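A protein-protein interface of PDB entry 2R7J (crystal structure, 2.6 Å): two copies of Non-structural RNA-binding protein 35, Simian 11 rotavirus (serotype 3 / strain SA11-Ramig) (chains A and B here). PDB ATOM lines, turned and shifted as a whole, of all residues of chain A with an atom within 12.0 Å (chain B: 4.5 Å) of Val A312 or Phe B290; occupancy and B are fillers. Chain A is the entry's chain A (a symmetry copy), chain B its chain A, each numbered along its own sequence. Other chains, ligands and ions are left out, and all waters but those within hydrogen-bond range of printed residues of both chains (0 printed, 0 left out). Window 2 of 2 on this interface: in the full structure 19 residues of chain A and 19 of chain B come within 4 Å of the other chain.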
ATOM      1  N   TRP A 211      14.796  -2.122   2.228  1.00  0.00           N
ATOM      2  CA  TRP A 211      15.925  -1.358   2.749  1.00  0.00           C
ATOM      3  C   TRP A 211      16.479  -0.320   1.795  1.00  0.00           C
ATOM      4  O   TRP A 211      16.509   0.877   2.099  1.00  0.00           O
ATOM      5  CB  TRP A 211      17.060  -2.303   3.147  1.00  0.00           C
ATOM      6  CG  TRP A 211      18.301  -1.583   3.547  1.00  0.00           C
ATOM      7  CD1 TRP A 211      19.418  -1.374   2.781  1.00  0.00           C
ATOM      8  CD2 TRP A 211      18.529  -0.898   4.787  1.00  0.00           C
ATOM      9  NE1 TRP A 211      20.326  -0.596   3.470  1.00  0.00           N
ATOM     10  CE2 TRP A 211      19.804  -0.289   4.702  1.00  0.00           C
ATOM     11  CE3 TRP A 211      17.777  -0.738   5.963  1.00  0.00           C
ATOM     12  CZ2 TRP A 211      20.345   0.470   5.749  1.00  0.00           C
ATOM     13  CZ3 TRP A 211      18.313   0.016   7.007  1.00  0.00           C
ATOM     14  CH2 TRP A 211      19.586   0.612   6.890  1.00  0.00           C
ATOM     15  N   GLY A 302      10.482  -8.193  10.212  1.00  0.00           N
ATOM     16  CA  GLY A 302      11.718  -8.161  10.964  1.00  0.00           C
ATOM     17  C   GLY A 302      12.904  -8.015  10.024  1.00  0.00           C
ATOM     18  O   GLY A 302      14.054  -7.972  10.465  1.00  0.00           O
ATOM     19  N   LEU A 303      12.629  -7.930   8.724  1.00  0.00           N
ATOM     20  CA  LEU A 303      13.683  -7.797   7.724  1.00  0.00           C
ATOM     21  C   LEU A 303      14.491  -6.504   7.857  1.00  0.00           C
ATOM     22  O   LEU A 303      15.726  -6.539   7.899  1.00  0.00           O
ATOM     23  CB  LEU A 303      13.091  -7.883   6.318  1.00  0.00           C
ATOM     24  CG  LEU A 303      12.489  -9.237   5.949  1.00  0.00           C
ATOM     25  CD1 LEU A 303      11.794  -9.150   4.604  1.00  0.00           C
ATOM     26  CD2 LEU A 303      13.580 -10.294   5.934  1.00  0.00           C
ATOM     27  N   SER A 304      13.802  -5.368   7.914  1.00  0.00           N
ATOM     28  CA  SER A 304      14.491  -4.093   8.033  1.00  0.00           C
ATOM     29  C   SER A 304      15.428  -4.130   9.233  1.00  0.00           C
ATOM     30  O   SER A 304      16.587  -3.726   9.139  1.00  0.00           O
ATOM     31  CB  SER A 304      13.486  -2.954   8.203  1.00  0.00           C
ATOM     32  OG  SER A 304      12.983  -2.910   9.530  1.00  0.00           O
ATOM     33  N   THR A 305      14.917  -4.622  10.358  1.00  0.00           N
ATOM     34  CA  THR A 305      15.704  -4.706  11.579  1.00  0.00           C
ATOM     35  C   THR A 305      16.984  -5.507  11.378  1.00  0.00           C
ATOM     36  O   THR A 305      18.051  -5.111  11.845  1.00  0.00           O
ATOM     37  CB  THR A 305      14.884  -5.334  12.712  1.00  0.00           C
ATOM     38  OG1 THR A 305      13.749  -4.505  12.981  1.00  0.00           O
ATOM     39  CG2 THR A 305      15.720  -5.454  13.980  1.00  0.00           C
ATOM     40  N   ASP A 306      16.881  -6.634  10.683  1.00  0.00           N
ATOM     41  CA  ASP A 306      18.056  -7.456  10.439  1.00  0.00           C
ATOM     42  C   ASP A 306      19.075  -6.667   9.629  1.00  0.00           C
ATOM     43  O   ASP A 306      20.229  -6.532  10.041  1.00  0.00           O
ATOM     44  CB  ASP A 306      17.681  -8.743   9.690  1.00  0.00           C
ATOM     45  CG  ASP A 306      16.742  -9.642  10.491  1.00  0.00           C
ATOM     46  OD1 ASP A 306      17.005  -9.867  11.698  1.00  0.00           O
ATOM     47  OD2 ASP A 306      15.745 -10.134   9.910  1.00  0.00           O
ATOM     48  N   ARG A 307      18.647  -6.139   8.483  1.00  0.00           N
ATOM     49  CA  ARG A 307      19.531  -5.367   7.614  1.00  0.00           C
ATOM     50  C   ARG A 307      20.107  -4.164   8.343  1.00  0.00           C
ATOM     51  O   ARG A 307      21.267  -3.791   8.147  1.00  0.00           O
ATOM     52  CB  ARG A 307      18.782  -4.902   6.359  1.00  0.00           C
ATOM     53  CG  ARG A 307      19.617  -4.023   5.433  1.00  0.00           C
ATOM     54  CD  ARG A 307      21.026  -4.589   5.228  1.00  0.00           C
ATOM     55  NE  ARG A 307      21.799  -3.850   4.232  1.00  0.00           N
ATOM     56  CZ  ARG A 307      21.552  -3.876   2.925  1.00  0.00           C
ATOM     57  NH1 ARG A 307      20.546  -4.607   2.455  1.00  0.00           N
ATOM     58  NH2 ARG A 307      22.313  -3.178   2.087  1.00  0.00           N
ATOM     59  N   LYS A 308      19.285  -3.560   9.189  1.00  0.00           N
ATOM     60  CA  LYS A 308      19.704  -2.411   9.969  1.00  0.00           C
ATOM     61  C   LYS A 308      20.849  -2.854  10.883  1.00  0.00           C
ATOM     62  O   LYS A 308      21.894  -2.202  10.959  1.00  0.00           O
ATOM     63  CB  LYS A 308      18.521  -1.903  10.788  1.00  0.00           C
ATOM     64  CG  LYS A 308      18.779  -0.625  11.528  1.00  0.00           C
ATOM     65  CD  LYS A 308      17.529  -0.153  12.252  1.00  0.00           C
ATOM     66  CE  LYS A 308      16.422   0.224  11.278  1.00  0.00           C
ATOM     67  NZ  LYS A 308      15.229   0.739  12.008  1.00  0.00           N
ATOM     68  N   MET A 309      20.653  -3.984  11.557  1.00  0.00           N
ATOM     69  CA  MET A 309      21.667  -4.533  12.455  1.00  0.00           C
ATOM     70  C   MET A 309      22.960  -4.907  11.723  1.00  0.00           C
ATOM     71  O   MET A 309      24.059  -4.713  12.257  1.00  0.00           O
ATOM     72  CB  MET A 309      21.119  -5.754  13.190  1.00  0.00           C
ATOM     73  CG  MET A 309      20.014  -5.434  14.179  1.00  0.00           C
ATOM     74  SD  MET A 309      20.492  -4.178  15.399  1.00  0.00           S
ATOM     75  CE  MET A 309      19.256  -2.921  15.053  1.00  0.00           C
ATOM     76  N   ASP A 310      22.842  -5.448  10.515  1.00  0.00           N
ATOM     77  CA  ASP A 310      24.042  -5.798   9.768  1.00  0.00           C
ATOM     78  C   ASP A 310      24.888  -4.532   9.652  1.00  0.00           C
ATOM     79  O   ASP A 310      26.033  -4.495  10.110  1.00  0.00           O
ATOM     80  CB  ASP A 310      23.704  -6.310   8.359  1.00  0.00           C
ATOM     81  CG  ASP A 310      22.794  -7.528   8.372  1.00  0.00           C
ATOM     82  OD1 ASP A 310      22.676  -8.165   9.443  1.00  0.00           O
ATOM     83  OD2 ASP A 310      22.206  -7.850   7.308  1.00  0.00           O
ATOM     84  N   GLU A 311      24.299  -3.499   9.049  1.00  0.00           N
ATOM     85  CA  GLU A 311      24.958  -2.211   8.850  1.00  0.00           C
ATOM     86  C   GLU A 311      25.728  -1.746  10.081  1.00  0.00           C
ATOM     87  O   GLU A 311      26.923  -1.448  10.007  1.00  0.00           O
ATOM     88  CB  GLU A 311      23.925  -1.150   8.477  1.00  0.00           C
ATOM     89  CG  GLU A 311      23.325  -1.321   7.102  1.00  0.00           C
ATOM     90  CD  GLU A 311      24.362  -1.183   6.004  1.00  0.00           C
ATOM     91  OE1 GLU A 311      25.202  -0.258   6.094  1.00  0.00           O
ATOM     92  OE2 GLU A 311      24.329  -1.990   5.045  1.00  0.00           O
ATOM     93  N   VAL A 312      25.033  -1.673  11.212  1.00  0.00           N
ATOM     94  CA  VAL A 312      25.645  -1.249  12.465  1.00  0.00           C
ATOM     95  C   VAL A 312      26.819  -2.154  12.850  1.00  0.00           C
ATOM     96  O   VAL A 312      27.862  -1.603  13.260  1.00  0.00           O
ATOM     97  CB  VAL A 312      24.617  -1.261  13.602  1.00  0.00           C
ATOM     98  CG1 VAL A 312      25.244  -0.717  14.878  1.00  0.00           C
ATOM     99  CG2 VAL A 312      23.396  -0.451  13.198  1.00  0.00           C
ATOM    100  N   TYR B 231      23.582   4.124   9.448  1.00  0.00           N
ATOM    101  CA  TYR B 231      23.658   3.058  10.443  1.00  0.00           C
ATOM    102  C   TYR B 231      25.054   2.453  10.499  1.00  0.00           C
ATOM    103  O   TYR B 231      25.491   1.991  11.542  1.00  0.00           O
ATOM    104  CB  TYR B 231      22.633   1.967  10.133  1.00  0.00           C
ATOM    105  CG  TYR B 231      21.254   2.286  10.668  1.00  0.00           C
ATOM    106  CD1 TYR B 231      20.956   2.124  12.022  1.00  0.00           C
ATOM    107  CD2 TYR B 231      20.256   2.775   9.832  1.00  0.00           C
ATOM    108  CE1 TYR B 231      19.694   2.445  12.523  1.00  0.00           C
ATOM    109  CE2 TYR B 231      18.994   3.094  10.325  1.00  0.00           C
ATOM    110  CZ  TYR B 231      18.724   2.927  11.664  1.00  0.00           C
ATOM    111  OH  TYR B 231      17.478   3.226  12.139  1.00  0.00           O
ATOM    112  N   VAL B 234      27.160   4.587  13.286  1.00  0.00           N
ATOM    113  CA  VAL B 234      26.840   4.814  14.691  1.00  0.00           C
ATOM    114  C   VAL B 234      27.887   4.265  15.654  1.00  0.00           C
ATOM    115  O   VAL B 234      27.958   4.678  16.813  1.00  0.00           O
ATOM    116  CB  VAL B 234      25.461   4.216  15.061  1.00  0.00           C
ATOM    117  CG1 VAL B 234      24.501   4.381  13.899  1.00  0.00           C
ATOM    118  CG2 VAL B 234      25.602   2.758  15.463  1.00  0.00           C
ATOM    119  N   TRP B 266      16.998   6.684  17.820  1.00  0.00           N
ATOM    120  CA  TRP B 266      16.968   5.267  17.496  1.00  0.00           C
ATOM    121  C   TRP B 266      17.047   4.489  18.806  1.00  0.00           C
ATOM    122  O   TRP B 266      17.818   4.833  19.701  1.00  0.00           O
ATOM    123  CB  TRP B 266      18.138   4.881  16.592  1.00  0.00           C
ATOM    124  CG  TRP B 266      18.196   3.391  16.294  1.00  0.00           C
ATOM    125  CD1 TRP B 266      17.141   2.569  15.994  1.00  0.00           C
ATOM    126  CD2 TRP B 266      19.374   2.577  16.199  1.00  0.00           C
ATOM    127  NE1 TRP B 266      17.591   1.298  15.712  1.00  0.00           N
ATOM    128  CE2 TRP B 266      18.956   1.274  15.831  1.00  0.00           C
ATOM    129  CE3 TRP B 266      20.742   2.821  16.387  1.00  0.00           C
ATOM    130  CZ2 TRP B 266      19.858   0.217  15.645  1.00  0.00           C
ATOM    131  CZ3 TRP B 266      21.647   1.766  16.203  1.00  0.00           C
ATOM    132  CH2 TRP B 266      21.195   0.477  15.835  1.00  0.00           C
ATOM    133  N   ASN B 268      18.301   1.447  19.978  1.00  0.00           N
ATOM    134  CA  ASN B 268      19.626   1.040  20.434  1.00  0.00           C
ATOM    135  C   ASN B 268      20.478   2.215  20.899  1.00  0.00           C
ATOM    136  O   ASN B 268      21.223   2.097  21.871  1.00  0.00           O
ATOM    137  CB  ASN B 268      20.360   0.291  19.317  1.00  0.00           C
ATOM    138  CG  ASN B 268      19.675  -1.011  18.945  1.00  0.00           C
ATOM    139  OD1 ASN B 268      18.446  -1.063  18.817  1.00  0.00           O
ATOM    140  ND2 ASN B 268      20.463  -2.066  18.759  1.00  0.00           N
ATOM    141  N   LYS B 286      28.280  -0.420  24.497  1.00  0.00           N
ATOM    142  CA  LYS B 286      28.259  -0.823  23.096  1.00  0.00           C
ATOM    143  C   LYS B 286      27.493  -2.124  22.863  1.00  0.00           C
ATOM    144  O   LYS B 286      27.044  -2.393  21.749  1.00  0.00           O
ATOM    145  CB  LYS B 286      29.689  -0.947  22.549  1.00  0.00           C
ATOM    146  CG  LYS B 286      30.447   0.375  22.506  1.00  0.00           C
ATOM    147  CD  LYS B 286      31.705   0.297  21.640  1.00  0.00           C
ATOM    148  CE  LYS B 286      31.367   0.225  20.152  1.00  0.00           C
ATOM    149  NZ  LYS B 286      32.577   0.166  19.282  1.00  0.00           N
ATOM    150  N   ARG B 287      27.345  -2.927  23.912  1.00  0.00           N
ATOM    151  CA  ARG B 287      26.615  -4.187  23.797  1.00  0.00           C
ATOM    152  C   ARG B 287      25.257  -3.894  23.165  1.00  0.00           C
ATOM    153  O   ARG B 287      24.892  -4.465  22.135  1.00  0.00           O
ATOM    154  CB  ARG B 287      26.381  -4.814  25.181  1.00  0.00           C
ATOM    155  CG  ARG B 287      27.641  -5.126  25.983  1.00  0.00           C
ATOM    156  CD  ARG B 287      28.304  -6.438  25.568  1.00  0.00           C
ATOM    157  NE  ARG B 287      29.529  -6.675  26.332  1.00  0.00           N
ATOM    158  CZ  ARG B 287      29.574  -6.824  27.654  1.00  0.00           C
ATOM    159  NH1 ARG B 287      28.459  -6.771  28.375  1.00  0.00           N
ATOM    160  NH2 ARG B 287      30.740  -7.007  28.262  1.00  0.00           N
ATOM    161  N   LEU B 288      24.530  -2.978  23.799  1.00  0.00           N
ATOM    162  CA  LEU B 288      23.192  -2.569  23.390  1.00  0.00           C
ATOM    163  C   LEU B 288      23.019  -2.040  21.959  1.00  0.00           C
ATOM    164  O   LEU B 288      21.906  -2.032  21.435  1.00  0.00           O
ATOM    165  CB  LEU B 288      22.661  -1.549  24.402  1.00  0.00           C
ATOM    166  CG  LEU B 288      22.707  -2.039  25.858  1.00  0.00           C
ATOM    167  CD1 LEU B 288      22.310  -0.923  26.821  1.00  0.00           C
ATOM    168  CD2 LEU B 288      21.794  -3.243  26.018  1.00  0.00           C
ATOM    169  N   LEU B 289      24.097  -1.604  21.316  1.00  0.00           N
ATOM    170  CA  LEU B 289      23.964  -1.116  19.946  1.00  0.00           C
ATOM    171  C   LEU B 289      23.766  -2.270  18.983  1.00  0.00           C
ATOM    172  O   LEU B 289      23.118  -2.130  17.954  1.00  0.00           O
ATOM    173  CB  LEU B 289      25.194  -0.306  19.517  1.00  0.00           C
ATOM    174  CG  LEU B 289      25.466   1.051  20.167  1.00  0.00           C
ATOM    175  CD1 LEU B 289      26.662   1.677  19.483  1.00  0.00           C
ATOM    176  CD2 LEU B 289      24.259   1.960  20.055  1.00  0.00           C
ATOM    177  N   PHE B 290      24.322  -3.421  19.325  1.00  0.00           N
ATOM    178  CA  PHE B 290      24.213  -4.580  18.455  1.00  0.00           C
ATOM    179  C   PHE B 290      23.105  -5.521  18.891  1.00  0.00           C
ATOM    180  O   PHE B 290      22.709  -6.423  18.152  1.00  0.00           O
ATOM    181  CB  PHE B 290      25.560  -5.302  18.421  1.00  0.00           C
ATOM    182  CG  PHE B 290      26.722  -4.391  18.100  1.00  0.00           C
ATOM    183  CD1 PHE B 290      27.164  -4.232  16.787  1.00  0.00           C
ATOM    184  CD2 PHE B 290      27.388  -3.711  19.115  1.00  0.00           C
ATOM    185  CE1 PHE B 290      28.259  -3.416  16.495  1.00  0.00           C
ATOM    186  CE2 PHE B 290      28.482  -2.893  18.831  1.00  0.00           C
ATOM    187  CZ  PHE B 290      28.918  -2.748  17.521  1.00  0.00           C
ATOM    188  N   GLN B 291      22.607  -5.298  20.100  1.00  0.00           N
ATOM    189  CA  GLN B 291      21.545  -6.123  20.651  1.00  0.00           C
ATOM    190  C   GLN B 291      20.207  -5.845  19.977  1.00  0.00           C
ATOM    191  O   GLN B 291      19.497  -4.902  20.335  1.00  0.00           O
ATOM    192  CB  GLN B 291      21.404  -5.891  22.159  1.00  0.00           C
ATOM    193  CG  GLN B 291      20.364  -6.799  22.809  1.00  0.00           C
ATOM    194  CD  GLN B 291      20.255  -6.597  24.307  1.00  0.00           C
ATOM    195  OE1 GLN B 291      21.231  -6.755  25.039  1.00  0.00           O
ATOM    196  NE2 GLN B 291      19.058  -6.252  24.773  1.00  0.00           N
ATOM    197  N   LYS B 292      19.871  -6.680  19.000  1.00  0.00           N
ATOM    198  CA  LYS B 292      18.618  -6.563  18.269  1.00  0.00           C
ATOM    199  C   LYS B 292      17.453  -6.594  19.259  1.00  0.00           C
ATOM    200  O   LYS B 292      17.066  -7.658  19.739  1.00  0.00           O
ATOM    201  CB  LYS B 292      18.503  -7.723  17.281  1.00  0.00           C
ATOM    202  CG  LYS B 292      17.253  -7.711  16.421  1.00  0.00           C
ATOM    203  CD  LYS B 292      17.362  -8.762  15.324  1.00  0.00           C
ATOM    204  CE  LYS B 292      18.623  -8.548  14.483  1.00  0.00           C
ATOM    205  NZ  LYS B 292      18.814  -9.607  13.453  1.00  0.00           N
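Trp A211 touches Tyr B231. Thr A305 touches Lys B292. Lys A308 touches Trp B266 (CD to NE1, 3.8 Å). Met A309 touches Trp B266. Met A309 touches Asn B268. O of Tyr B231 touches CA of Val A312, 3.4 Å away. CG2 of Val B234 touches CG1 of Val A312, 3.5 Å away. Val A312 touches Trp B266. CG1 of Val A312 touches O of Leu B289, 3.997 Å away. O of Val A312 touches CE1 of Phe B290 (3.7 Å).
Of the 12 printed residues of chain A, 7 touch a printed residue of chain B. Along chain A the printed residues that touch a printed residue of chain B span positions 211 to 312. Of the 11 printed residues of chain B, 7 touch a printed residue of chain A.
No position is printed for both chains.
The side-chain amide nitrogen (ND2) of Asn B268 lies within hydrogen-bond range of the backbone carbonyl oxygen (O) of Gln B291, at 3.4 Å. The side-chain amide nitrogen (ND2) of Asn B268 lies within hydrogen-bond range of the backbone carbonyl oxygen (O) of Leu B288. The backbone carbonyl oxygen (O) of Leu B289 sits at hydrogen-bond distance from the side-chain amide nitrogen (ND2) of Asn B268, at 2.8 Å. The guanidinium group (NE) of Arg A307 is in salt-bridge range of the side-chain carboxylate (OE2) of Glu A311, 3.2 Å away.
The side-chain hydroxyl of Tyr B231 lies close to the side-chain amino group of Lys A308, 3.4 Å away. The side-chain amino group of Lys B292 lies within salt-bridge range of the side-chain carboxylate of Asp A306 (2.5 Å).
Of the printed residues of chain B, Trp A211 touches Tyr B231. Printed residues of chain B within 4 Å of Lys A308: Tyr B231 (3.3 Å) and Trp B266 (3.8 Å). Printed residues of chain B within 4 Å of Glu A311: Tyr B231. Printed residues of chain B within 4 Å of Val A312: Tyr B231 (3.4 Å), Val B234 (3.5 Å), Trp B266 (3.6 Å), Leu B289 (3.997 Å) and Phe B290 (3.7 Å). Of chain A, only Val A312 comes within 4 Å of Val B234. Asn B268 touches just one residue of chain A: Met A309 (3.97 Å). Lys B286 touches none of the printed residues of chain A. Arg B287 touches none of the printed residues of chain A. Of the printed residues of chain A, Leu B289 touches Val A312. Of chain A, only Val A312 (3.7 Å) comes within 4 Å of Phe B290. No residue of chain A comes within 4 Å of Gln B291. The nearest printed residue of chain B that does not touch Asp A306 is Phe B290 (8.5 Å).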
